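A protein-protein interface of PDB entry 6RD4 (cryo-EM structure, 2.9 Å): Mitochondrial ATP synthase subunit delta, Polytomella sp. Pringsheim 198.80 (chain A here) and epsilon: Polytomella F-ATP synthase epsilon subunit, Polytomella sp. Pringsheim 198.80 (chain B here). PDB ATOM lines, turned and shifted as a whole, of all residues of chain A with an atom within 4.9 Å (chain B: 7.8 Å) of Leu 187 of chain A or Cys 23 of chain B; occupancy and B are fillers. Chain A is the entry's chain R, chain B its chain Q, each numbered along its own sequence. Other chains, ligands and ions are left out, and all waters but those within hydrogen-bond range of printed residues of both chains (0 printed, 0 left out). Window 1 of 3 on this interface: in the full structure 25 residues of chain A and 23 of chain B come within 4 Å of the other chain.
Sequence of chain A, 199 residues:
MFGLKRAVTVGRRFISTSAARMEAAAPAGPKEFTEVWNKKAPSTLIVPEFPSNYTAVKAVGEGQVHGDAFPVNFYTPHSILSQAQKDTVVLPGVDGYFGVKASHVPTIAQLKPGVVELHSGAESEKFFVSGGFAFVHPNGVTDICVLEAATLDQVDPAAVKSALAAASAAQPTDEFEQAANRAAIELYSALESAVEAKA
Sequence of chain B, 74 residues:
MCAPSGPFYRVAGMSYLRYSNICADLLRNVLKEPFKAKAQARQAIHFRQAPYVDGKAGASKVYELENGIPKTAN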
ATOM      1  N   PRO A 113     -13.539 -31.371  14.565  1.00  0.00           N
ATOM      2  CA  PRO A 113     -13.146 -32.496  13.714  1.00  0.00           C
ATOM      3  C   PRO A 113     -12.266 -33.477  14.458  1.00  0.00           C
ATOM      4  O   PRO A 113     -11.125 -33.161  14.793  1.00  0.00           O
ATOM      5  CB  PRO A 113     -12.385 -31.812  12.579  1.00  0.00           C
ATOM      6  CG  PRO A 113     -13.000 -30.491  12.479  1.00  0.00           C
ATOM      7  CD  PRO A 113     -13.418 -30.089  13.852  1.00  0.00           C
ATOM      8  N   PHE A 128     -14.195 -41.036  12.293  1.00  0.00           N
ATOM      9  CA  PHE A 128     -13.707 -39.665  12.272  1.00  0.00           C
ATOM     10  C   PHE A 128     -14.804 -38.762  11.732  1.00  0.00           C
ATOM     11  O   PHE A 128     -15.302 -38.986  10.627  1.00  0.00           O
ATOM     12  CB  PHE A 128     -12.458 -39.549  11.404  1.00  0.00           C
ATOM     13  CG  PHE A 128     -11.906 -38.163  11.317  1.00  0.00           C
ATOM     14  CD1 PHE A 128     -11.131 -37.650  12.335  1.00  0.00           C
ATOM     15  CD2 PHE A 128     -12.150 -37.375  10.211  1.00  0.00           C
ATOM     16  CE1 PHE A 128     -10.620 -36.377  12.254  1.00  0.00           C
ATOM     17  CE2 PHE A 128     -11.645 -36.103  10.124  1.00  0.00           C
ATOM     18  CZ  PHE A 128     -10.877 -35.603  11.146  1.00  0.00           C
ATOM     19  N   SER A 130     -16.594 -34.684  11.175  1.00  0.00           N
ATOM     20  CA  SER A 130     -16.193 -33.377  10.682  1.00  0.00           C
ATOM     21  C   SER A 130     -16.497 -32.253  11.653  1.00  0.00           C
ATOM     22  O   SER A 130     -16.182 -31.098  11.357  1.00  0.00           O
ATOM     23  CB  SER A 130     -16.896 -33.082   9.365  1.00  0.00           C
ATOM     24  OG  SER A 130     -18.283 -32.914   9.588  1.00  0.00           O
ATOM     25  N   ALA A 183     -10.577 -23.569   9.214  1.00  0.00           N
ATOM     26  CA  ALA A 183     -11.307 -24.826   9.284  1.00  0.00           C
ATOM     27  C   ALA A 183     -10.639 -25.900   8.445  1.00  0.00           C
ATOM     28  O   ALA A 183     -10.723 -27.091   8.766  1.00  0.00           O
ATOM     29  CB  ALA A 183     -12.744 -24.609   8.830  1.00  0.00           C
ATOM     30  N   ALA A 184      -9.958 -25.498   7.371  1.00  0.00           N
ATOM     31  CA  ALA A 184      -9.243 -26.461   6.544  1.00  0.00           C
ATOM     32  C   ALA A 184      -8.020 -27.005   7.266  1.00  0.00           C
ATOM     33  O   ALA A 184      -7.696 -28.190   7.153  1.00  0.00           O
ATOM     34  CB  ALA A 184      -8.838 -25.817   5.220  1.00  0.00           C
ATOM     35  N   ILE A 185      -7.329 -26.146   8.010  1.00  0.00           N
ATOM     36  CA  ILE A 185      -6.094 -26.568   8.659  1.00  0.00           C
ATOM     37  C   ILE A 185      -6.388 -27.469   9.853  1.00  0.00           C
ATOM     38  O   ILE A 185      -5.779 -28.535  10.000  1.00  0.00           O
ATOM     39  CB  ILE A 185      -5.250 -25.342   9.053  1.00  0.00           C
ATOM     40  CG1 ILE A 185      -4.746 -24.622   7.806  1.00  0.00           C
ATOM     41  CG2 ILE A 185      -4.059 -25.751   9.857  1.00  0.00           C
ATOM     42  CD1 ILE A 185      -4.126 -23.275   8.092  1.00  0.00           C
ATOM     43  N   GLU A 186      -7.349 -27.082  10.698  1.00  0.00           N
ATOM     44  CA  GLU A 186      -7.578 -27.817  11.940  1.00  0.00           C
ATOM     45  C   GLU A 186      -8.231 -29.167  11.678  1.00  0.00           C
ATOM     46  O   GLU A 186      -8.158 -30.072  12.515  1.00  0.00           O
ATOM     47  CB  GLU A 186      -8.434 -26.992  12.902  1.00  0.00           C
ATOM     48  CG  GLU A 186      -9.908 -26.909  12.531  1.00  0.00           C
ATOM     49  CD  GLU A 186     -10.732 -26.102  13.518  1.00  0.00           C
ATOM     50  OE1 GLU A 186     -10.145 -25.495  14.437  1.00  0.00           O
ATOM     51  OE2 GLU A 186     -11.971 -26.087  13.376  1.00  0.00           O
ATOM     52  N   LEU A 187      -8.870 -29.324  10.520  1.00  0.00           N
ATOM     53  CA  LEU A 187      -9.493 -30.595  10.191  1.00  0.00           C
ATOM     54  C   LEU A 187      -8.451 -31.614   9.762  1.00  0.00           C
ATOM     55  O   LEU A 187      -8.451 -32.751  10.251  1.00  0.00           O
ATOM     56  CB  LEU A 187     -10.546 -30.382   9.107  1.00  0.00           C
ATOM     57  CG  LEU A 187     -11.133 -31.503   8.257  1.00  0.00           C
ATOM     58  CD1 LEU A 187     -11.657 -32.676   9.039  1.00  0.00           C
ATOM     59  CD2 LEU A 187     -12.268 -30.894   7.510  1.00  0.00           C
ATOM     60  N   TYR A 188      -7.553 -31.226   8.860  1.00  0.00           N
ATOM     61  CA  TYR A 188      -6.536 -32.160   8.400  1.00  0.00           C
ATOM     62  C   TYR A 188      -5.507 -32.431   9.483  1.00  0.00           C
ATOM     63  O   TYR A 188      -4.966 -33.536   9.550  1.00  0.00           O
ATOM     64  CB  TYR A 188      -5.848 -31.619   7.155  1.00  0.00           C
ATOM     65  CG  TYR A 188      -6.762 -31.473   5.977  1.00  0.00           C
ATOM     66  CD1 TYR A 188      -7.786 -32.380   5.752  1.00  0.00           C
ATOM     67  CD2 TYR A 188      -6.616 -30.412   5.099  1.00  0.00           C
ATOM     68  CE1 TYR A 188      -8.633 -32.232   4.681  1.00  0.00           C
ATOM     69  CE2 TYR A 188      -7.459 -30.260   4.022  1.00  0.00           C
ATOM     70  CZ  TYR A 188      -8.462 -31.174   3.817  1.00  0.00           C
ATOM     71  OH  TYR A 188      -9.301 -31.027   2.740  1.00  0.00           O
ATOM     72  N   SER A 189      -5.247 -31.444  10.347  1.00  0.00           N
ATOM     73  CA  SER A 189      -4.257 -31.606  11.405  1.00  0.00           C
ATOM     74  C   SER A 189      -4.711 -32.622  12.438  1.00  0.00           C
ATOM     75  O   SER A 189      -3.907 -33.423  12.925  1.00  0.00           O
ATOM     76  CB  SER A 189      -4.004 -30.271  12.080  1.00  0.00           C
ATOM     77  OG  SER A 189      -3.818 -29.259  11.110  1.00  0.00           O
ATOM     78  N   ALA A 190      -5.994 -32.599  12.787  1.00  0.00           N
ATOM     79  CA  ALA A 190      -6.538 -33.663  13.617  1.00  0.00           C
ATOM     80  C   ALA A 190      -6.640 -34.959  12.829  1.00  0.00           C
ATOM     81  O   ALA A 190      -6.584 -36.050  13.407  1.00  0.00           O
ATOM     82  CB  ALA A 190      -7.902 -33.257  14.162  1.00  0.00           C
ATOM     83  N   LEU A 191      -6.795 -34.853  11.509  1.00  0.00           N
ATOM     84  CA  LEU A 191      -6.827 -36.044  10.674  1.00  0.00           C
ATOM     85  C   LEU A 191      -5.439 -36.629  10.490  1.00  0.00           C
ATOM     86  O   LEU A 191      -5.312 -37.845  10.328  1.00  0.00           O
ATOM     87  CB  LEU A 191      -7.464 -35.720   9.324  1.00  0.00           C
ATOM     88  CG  LEU A 191      -7.922 -36.866   8.426  1.00  0.00           C
ATOM     89  CD1 LEU A 191      -8.640 -37.932   9.223  1.00  0.00           C
ATOM     90  CD2 LEU A 191      -8.824 -36.321   7.347  1.00  0.00           C
ATOM     91  N   PHE B   8     -14.796 -18.470  15.236  1.00  0.00           N
ATOM     92  CA  PHE B   8     -14.016 -17.897  14.150  1.00  0.00           C
ATOM     93  C   PHE B   8     -14.785 -17.844  12.846  1.00  0.00           C
ATOM     94  O   PHE B   8     -14.439 -17.049  11.968  1.00  0.00           O
ATOM     95  CB  PHE B   8     -12.711 -18.665  13.955  1.00  0.00           C
ATOM     96  CG  PHE B   8     -12.885 -20.097  13.549  1.00  0.00           C
ATOM     97  CD1 PHE B   8     -12.798 -20.468  12.220  1.00  0.00           C
ATOM     98  CD2 PHE B   8     -13.074 -21.082  14.501  1.00  0.00           C
ATOM     99  CE1 PHE B   8     -12.933 -21.783  11.850  1.00  0.00           C
ATOM    100  CE2 PHE B   8     -13.212 -22.396  14.138  1.00  0.00           C
ATOM    101  CZ  PHE B   8     -13.137 -22.747  12.812  1.00  0.00           C
ATOM    102  N   TYR B   9     -15.808 -18.671  12.694  1.00  0.00           N
ATOM    103  CA  TYR B   9     -16.680 -18.562  11.540  1.00  0.00           C
ATOM    104  C   TYR B   9     -17.723 -17.478  11.738  1.00  0.00           C
ATOM    105  O   TYR B   9     -18.071 -16.775  10.790  1.00  0.00           O
ATOM    106  CB  TYR B   9     -17.354 -19.907  11.255  1.00  0.00           C
ATOM    107  CG  TYR B   9     -17.951 -20.595  12.457  1.00  0.00           C
ATOM    108  CD1 TYR B   9     -17.222 -21.522  13.178  1.00  0.00           C
ATOM    109  CD2 TYR B   9     -19.253 -20.337  12.850  1.00  0.00           C
ATOM    110  CE1 TYR B   9     -17.765 -22.153  14.264  1.00  0.00           C
ATOM    111  CE2 TYR B   9     -19.798 -20.961  13.937  1.00  0.00           C
ATOM    112  CZ  TYR B   9     -19.053 -21.865  14.638  1.00  0.00           C
ATOM    113  OH  TYR B   9     -19.602 -22.491  15.721  1.00  0.00           O
ATOM    114  N   TYR B  16     -23.025 -21.049  10.782  1.00  0.00           N
ATOM    115  CA  TYR B  16     -22.541 -22.352  11.220  1.00  0.00           C
ATOM    116  C   TYR B  16     -22.807 -23.417  10.168  1.00  0.00           C
ATOM    117  O   TYR B  16     -22.022 -24.360  10.026  1.00  0.00           O
ATOM    118  CB  TYR B  16     -23.182 -22.744  12.547  1.00  0.00           C
ATOM    119  CG  TYR B  16     -22.809 -24.136  12.968  1.00  0.00           C
ATOM    120  CD1 TYR B  16     -21.554 -24.405  13.469  1.00  0.00           C
ATOM    121  CD2 TYR B  16     -23.698 -25.192  12.829  1.00  0.00           C
ATOM    122  CE1 TYR B  16     -21.198 -25.674  13.829  1.00  0.00           C
ATOM    123  CE2 TYR B  16     -23.340 -26.461  13.174  1.00  0.00           C
ATOM    124  CZ  TYR B  16     -22.095 -26.694  13.682  1.00  0.00           C
ATOM    125  OH  TYR B  16     -21.739 -27.959  14.048  1.00  0.00           O
ATOM    126  N   LEU B  17     -23.902 -23.278   9.423  1.00  0.00           N
ATOM    127  CA  LEU B  17     -24.259 -24.264   8.408  1.00  0.00           C
ATOM    128  C   LEU B  17     -23.250 -24.288   7.280  1.00  0.00           C
ATOM    129  O   LEU B  17     -22.943 -25.355   6.740  1.00  0.00           O
ATOM    130  CB  LEU B  17     -25.631 -23.957   7.838  1.00  0.00           C
ATOM    131  CG  LEU B  17     -26.793 -24.268   8.741  1.00  0.00           C
ATOM    132  CD1 LEU B  17     -27.952 -23.497   8.203  1.00  0.00           C
ATOM    133  CD2 LEU B  17     -27.052 -25.747   8.704  1.00  0.00           C
ATOM    134  N   ARG B  18     -22.733 -23.122   6.902  1.00  0.00           N
ATOM    135  CA  ARG B  18     -21.710 -23.105   5.874  1.00  0.00           C
ATOM    136  C   ARG B  18     -20.406 -23.660   6.402  1.00  0.00           C
ATOM    137  O   ARG B  18     -19.739 -24.430   5.711  1.00  0.00           O
ATOM    138  CB  ARG B  18     -21.498 -21.698   5.341  1.00  0.00           C
ATOM    139  CG  ARG B  18     -20.696 -21.708   4.067  1.00  0.00           C
ATOM    140  CD  ARG B  18     -20.580 -20.340   3.486  1.00  0.00           C
ATOM    141  NE  ARG B  18     -21.839 -19.903   2.913  1.00  0.00           N
ATOM    142  CZ  ARG B  18     -22.127 -19.998   1.626  1.00  0.00           C
ATOM    143  NH1 ARG B  18     -21.247 -20.521   0.785  1.00  0.00           N
ATOM    144  NH2 ARG B  18     -23.297 -19.572   1.183  1.00  0.00           N
ATOM    145  N   TYR B  19     -20.058 -23.316   7.641  1.00  0.00           N
ATOM    146  CA  TYR B  19     -18.817 -23.787   8.241  1.00  0.00           C
ATOM    147  C   TYR B  19     -18.835 -25.294   8.422  1.00  0.00           C
ATOM    148  O   TYR B  19     -17.847 -25.978   8.141  1.00  0.00           O
ATOM    149  CB  TYR B  19     -18.592 -23.089   9.580  1.00  0.00           C
ATOM    150  CG  TYR B  19     -17.704 -23.862  10.518  1.00  0.00           C
ATOM    151  CD1 TYR B  19     -18.229 -24.506  11.628  1.00  0.00           C
ATOM    152  CD2 TYR B  19     -16.343 -23.949  10.294  1.00  0.00           C
ATOM    153  CE1 TYR B  19     -17.429 -25.219  12.469  1.00  0.00           C
ATOM    154  CE2 TYR B  19     -15.539 -24.659  11.134  1.00  0.00           C
ATOM    155  CZ  TYR B  19     -16.085 -25.292  12.221  1.00  0.00           C
ATOM    156  OH  TYR B  19     -15.275 -26.004  13.073  1.00  0.00           O
ATOM    157  N   SER B  20     -19.957 -25.830   8.883  1.00  0.00           N
ATOM    158  CA  SER B  20     -20.007 -27.253   9.160  1.00  0.00           C
ATOM    159  C   SER B  20     -20.095 -28.061   7.881  1.00  0.00           C
ATOM    160  O   SER B  20     -19.764 -29.249   7.883  1.00  0.00           O
ATOM    161  CB  SER B  20     -21.180 -27.559  10.072  1.00  0.00           C
ATOM    162  OG  SER B  20     -21.467 -28.933  10.044  1.00  0.00           O
ATOM    163  N   ASN B  21     -20.527 -27.439   6.784  1.00  0.00           N
ATOM    164  CA  ASN B  21     -20.531 -28.115   5.494  1.00  0.00           C
ATOM    165  C   ASN B  21     -19.202 -27.997   4.767  1.00  0.00           C
ATOM    166  O   ASN B  21     -18.868 -28.888   3.983  1.00  0.00           O
ATOM    167  CB  ASN B  21     -21.650 -27.576   4.611  1.00  0.00           C
ATOM    168  CG  ASN B  21     -22.920 -28.354   4.769  1.00  0.00           C
ATOM    169  OD1 ASN B  21     -23.058 -29.434   4.213  1.00  0.00           O
ATOM    170  ND2 ASN B  21     -23.860 -27.815   5.521  1.00  0.00           N
ATOM    171  N   ILE B  22     -18.454 -26.909   4.982  1.00  0.00           N
ATOM    172  CA  ILE B  22     -17.081 -26.844   4.488  1.00  0.00           C
ATOM    173  C   ILE B  22     -16.246 -27.946   5.121  1.00  0.00           C
ATOM    174  O   ILE B  22     -15.556 -28.695   4.428  1.00  0.00           O
ATOM    175  CB  ILE B  22     -16.465 -25.456   4.738  1.00  0.00           C
ATOM    176  CG1 ILE B  22     -17.153 -24.384   3.904  1.00  0.00           C
ATOM    177  CG2 ILE B  22     -15.003 -25.462   4.420  1.00  0.00           C
ATOM    178  CD1 ILE B  22     -16.739 -22.990   4.266  1.00  0.00           C
ATOM    179  N   CYS B  23     -16.353 -28.103   6.439  1.00  0.00           N
ATOM    180  CA  CYS B  23     -15.667 -29.196   7.117  1.00  0.00           C
ATOM    181  C   CYS B  23     -16.223 -30.554   6.719  1.00  0.00           C
ATOM    182  O   CYS B  23     -15.517 -31.558   6.817  1.00  0.00           O
ATOM    183  CB  CYS B  23     -15.757 -29.015   8.629  1.00  0.00           C
ATOM    184  SG  CYS B  23     -14.866 -27.588   9.225  1.00  0.00           S
ATOM    185  N   ALA B  24     -17.473 -30.611   6.273  1.00  0.00           N
ATOM    186  CA  ALA B  24     -17.977 -31.851   5.700  1.00  0.00           C
ATOM    187  C   ALA B  24     -17.422 -32.070   4.303  1.00  0.00           C
ATOM    188  O   ALA B  24     -17.176 -33.211   3.901  1.00  0.00           O
ATOM    189  CB  ALA B  24     -19.500 -31.835   5.678  1.00  0.00           C
ATOM    190  N   ASP B  25     -17.208 -30.982   3.554  1.00  0.00           N
ATOM    191  CA  ASP B  25     -16.682 -31.083   2.195  1.00  0.00           C
ATOM    192  C   ASP B  25     -15.240 -31.558   2.201  1.00  0.00           C
ATOM    193  O   ASP B  25     -14.847 -32.411   1.396  1.00  0.00           O
ATOM    194  CB  ASP B  25     -16.770 -29.732   1.492  1.00  0.00           C
ATOM    195  CG  ASP B  25     -18.123 -29.473   0.880  1.00  0.00           C
ATOM    196  OD1 ASP B  25     -18.970 -30.391   0.878  1.00  0.00           O
ATOM    197  OD2 ASP B  25     -18.333 -28.351   0.385  1.00  0.00           O
ATOM    198  N   LEU B  26     -14.432 -31.008   3.104  1.00  0.00           N
ATOM    199  CA  LEU B  26     -13.011 -31.310   3.108  1.00  0.00           C
ATOM    200  C   LEU B  26     -12.724 -32.704   3.633  1.00  0.00           C
ATOM    201  O   LEU B  26     -11.674 -33.268   3.320  1.00  0.00           O
ATOM    202  CB  LEU B  26     -12.268 -30.263   3.924  1.00  0.00           C
ATOM    203  CG  LEU B  26     -12.511 -28.845   3.427  1.00  0.00           C
ATOM    204  CD1 LEU B  26     -11.851 -27.849   4.327  1.00  0.00           C
ATOM    205  CD2 LEU B  26     -11.995 -28.708   2.012  1.00  0.00           C
ATOM    206  N   LEU B  27     -13.632 -33.279   4.418  1.00  0.00           N
ATOM    207  CA  LEU B  27     -13.464 -34.680   4.777  1.00  0.00           C
ATOM    208  C   LEU B  27     -13.688 -35.588   3.575  1.00  0.00           C
ATOM    209  O   LEU B  27     -12.993 -36.594   3.433  1.00  0.00           O
ATOM    210  CB  LEU B  27     -14.406 -35.050   5.920  1.00  0.00           C
ATOM    211  CG  LEU B  27     -14.372 -36.475   6.478  1.00  0.00           C
ATOM    212  CD1 LEU B  27     -12.967 -36.951   6.716  1.00  0.00           C
ATOM    213  CD2 LEU B  27     -15.117 -36.519   7.777  1.00  0.00           C
ATOM    214  N   ARG B  28     -14.616 -35.232   2.683  1.00  0.00           N
ATOM    215  CA  ARG B  28     -14.940 -36.109   1.561  1.00  0.00           C
ATOM    216  C   ARG B  28     -13.825 -36.159   0.527  1.00  0.00           C
ATOM    217  O   ARG B  28     -13.662 -37.179  -0.150  1.00  0.00           O
ATOM    218  CB  ARG B  28     -16.244 -35.665   0.901  1.00  0.00           C
ATOM    219  CG  ARG B  28     -17.456 -35.748   1.804  1.00  0.00           C
ATOM    220  CD  ARG B  28     -18.721 -35.402   1.055  1.00  0.00           C
ATOM    221  NE  ARG B  28     -19.809 -35.094   1.970  1.00  0.00           N
ATOM    222  CZ  ARG B  28     -20.250 -33.868   2.197  1.00  0.00           C
ATOM    223  NH1 ARG B  28     -19.701 -32.843   1.564  1.00  0.00           N
ATOM    224  NH2 ARG B  28     -21.239 -33.667   3.054  1.00  0.00           N
ATOM    225  N   ASN B  29     -13.020 -35.098   0.421  1.00  0.00           N
ATOM    226  CA  ASN B  29     -11.917 -35.069  -0.536  1.00  0.00           C
ATOM    227  C   ASN B  29     -10.756 -35.969  -0.123  1.00  0.00           C
ATOM    228  O   ASN B  29      -9.807 -36.131  -0.894  1.00  0.00           O
ATOM    229  CB  ASN B  29     -11.407 -33.639  -0.702  1.00  0.00           C
ATOM    230  CG  ASN B  29     -12.476 -32.690  -1.193  1.00  0.00           C
ATOM    231  OD1 ASN B  29     -13.640 -33.058  -1.310  1.00  0.00           O
ATOM    232  ND2 ASN B  29     -12.089 -31.453  -1.455  1.00  0.00           N
ATOM    233  N   VAL B  30     -10.805 -36.534   1.080  1.00  0.00           N
ATOM    234  CA  VAL B  30      -9.738 -37.319   1.678  1.00  0.00           C
ATOM    235  C   VAL B  30     -10.158 -38.792   1.803  1.00  0.00           C
ATOM    236  O   VAL B  30      -9.364 -39.649   2.211  1.00  0.00           O
ATOM    237  CB  VAL B  30      -9.345 -36.658   3.025  1.00  0.00           C
ATOM    238  CG1 VAL B  30      -8.170 -37.272   3.757  1.00  0.00           C
ATOM    239  CG2 VAL B  30      -9.022 -35.199   2.796  1.00  0.00           C
ATOM    240  N   ILE B  69     -20.257 -27.003  -1.235  1.00  0.00           N
ATOM    241  CA  ILE B  69     -20.684 -25.657  -0.841  1.00  0.00           C
ATOM    242  C   ILE B  69     -19.503 -24.705  -1.017  1.00  0.00           C
ATOM    243  O   ILE B  69     -18.343 -25.141  -0.872  1.00  0.00           O
ATOM    244  CB  ILE B  69     -21.216 -25.695   0.612  1.00  0.00           C
ATOM    245  CG1 ILE B  69     -22.034 -24.472   1.009  1.00  0.00           C
ATOM    246  CG2 ILE B  69     -20.127 -25.917   1.647  1.00  0.00           C
ATOM    247  CD1 ILE B  69     -22.750 -24.660   2.315  1.00  0.00           C
ATOM    248  N   LYS B  71     -16.425 -22.432  -0.701  1.00  0.00           N
ATOM    249  CA  LYS B  71     -15.472 -22.072   0.339  1.00  0.00           C
ATOM    250  C   LYS B  71     -15.219 -20.577   0.408  1.00  0.00           C
ATOM    251  O   LYS B  71     -14.803 -20.081   1.461  1.00  0.00           O
ATOM    252  CB  LYS B  71     -14.145 -22.788   0.099  1.00  0.00           C
ATOM    253  CG  LYS B  71     -14.246 -24.292   0.058  1.00  0.00           C
ATOM    254  CD  LYS B  71     -13.054 -24.897  -0.657  1.00  0.00           C
ATOM    255  CE  LYS B  71     -13.137 -26.410  -0.662  1.00  0.00           C
ATOM    256  NZ  LYS B  71     -14.449 -26.913  -1.139  1.00  0.00           N
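The side-chain hydroxyl of Tyr 19 of chain B is in hydrogen-bond range of the side-chain carboxylate of Glu 186 of chain A (3.3 Å).
The side-chain hydroxyl (OH) of Tyr 188 of chain A sits close to the backbone carbonyl oxygen (O) of Leu 26 of chain B (3.3 Å).
SG of Cys 23 of chain B is in hydrogen-bond range of O of Tyr 19 of chain B.
Among the printed residues, merely in contact across the chains: Ser 130 of chain A with Cys 23 of chain B (3.3 Å), Leu 187 of chain A with Cys 23 of chain B (3.4 Å), Tyr 188 of chain A with Val 30 of chain B (3.5 Å), Glu 186 of chain A with Phe 8 of chain B (3.6 Å), Phe 128 of chain A with Leu 27 of chain B (3.6 Å), Ala 183 of chain A with Tyr 19 of chain B (3.6 Å), Leu 187 of chain A with Leu 26 of chain B (3.6 Å), Ala 183 of chain A with Cys 23 of chain B (3.7 Å), Ala 184 of chain A with Leu 26 of chain B (3.7 Å), Leu 191 of chain A with Val 30 of chain B (3.8 Å), Ala 183 of chain A with Phe 8 of chain B (3.96 Å) and Ser 130 of chain A with Ala 24 of chain B (3.9999 Å).
Of the printed residues of chain B, Phe 128 of chain A touches Leu 27 (3.6 Å).
Of the printed residues of chain B, Glu 186 of chain A touches Phe 8 (3.6 Å) and Tyr 19 (3.3 Å).
Leu 187 of chain A touches just these residues of chain B: Cys 23 (3.4 Å) and Leu 26 (3.6 Å).
Of the printed residues of chain B, Tyr 188 of chain A touches Leu 26 (3.3 Å) and Val 30 (3.5 Å).
Ala 190 of chain A touches none of the printed residues of chain B.
Leu 17 of chain B touches none of the printed residues of chain A.
Of the printed residues of chain A, Tyr 19 of chain B touches Ala 183 (3.6 Å) and Glu 186 (3.3 Å).
Cys 23 of chain B touches just these residues of chain A: Ser 130 (3.3 Å), Ala 183 (3.7 Å) and Leu 187 (3.4 Å).
The nearest residue of chain A that does not touch Cys 23 of chain B is Pro 113 of chain A (4.7 Å).
The nearest printed residue of chain A that does not touch Ala 24 of chain B is Leu 187 of chain A (5.4 Å).
Of the 12 printed residues of chain A, 8 touch a printed residue of chain B.
Printed residues of chain A that touch a printed residue of chain B: Phe 128, Ser 130, Ala 183, Ala 184, Glu 186, Leu 187, Tyr 188 and Leu 191.
Printed residues of chain B that touch a printed residue of chain A: Phe 8, Tyr 19, Cys 23, Ala 24, Leu 26, Leu 27 and Val 30.
Hydrophobic or aromatic side chains of chain B within 4 Å of the printed part of chain A: Phe 8, Tyr 19, Leu 26, Leu 27 and Val 30.
Among the printed residues, no Asp or Glu carboxylate lies within 4 Å of a Lys or Arg side-chain nitrogen of the other chain.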
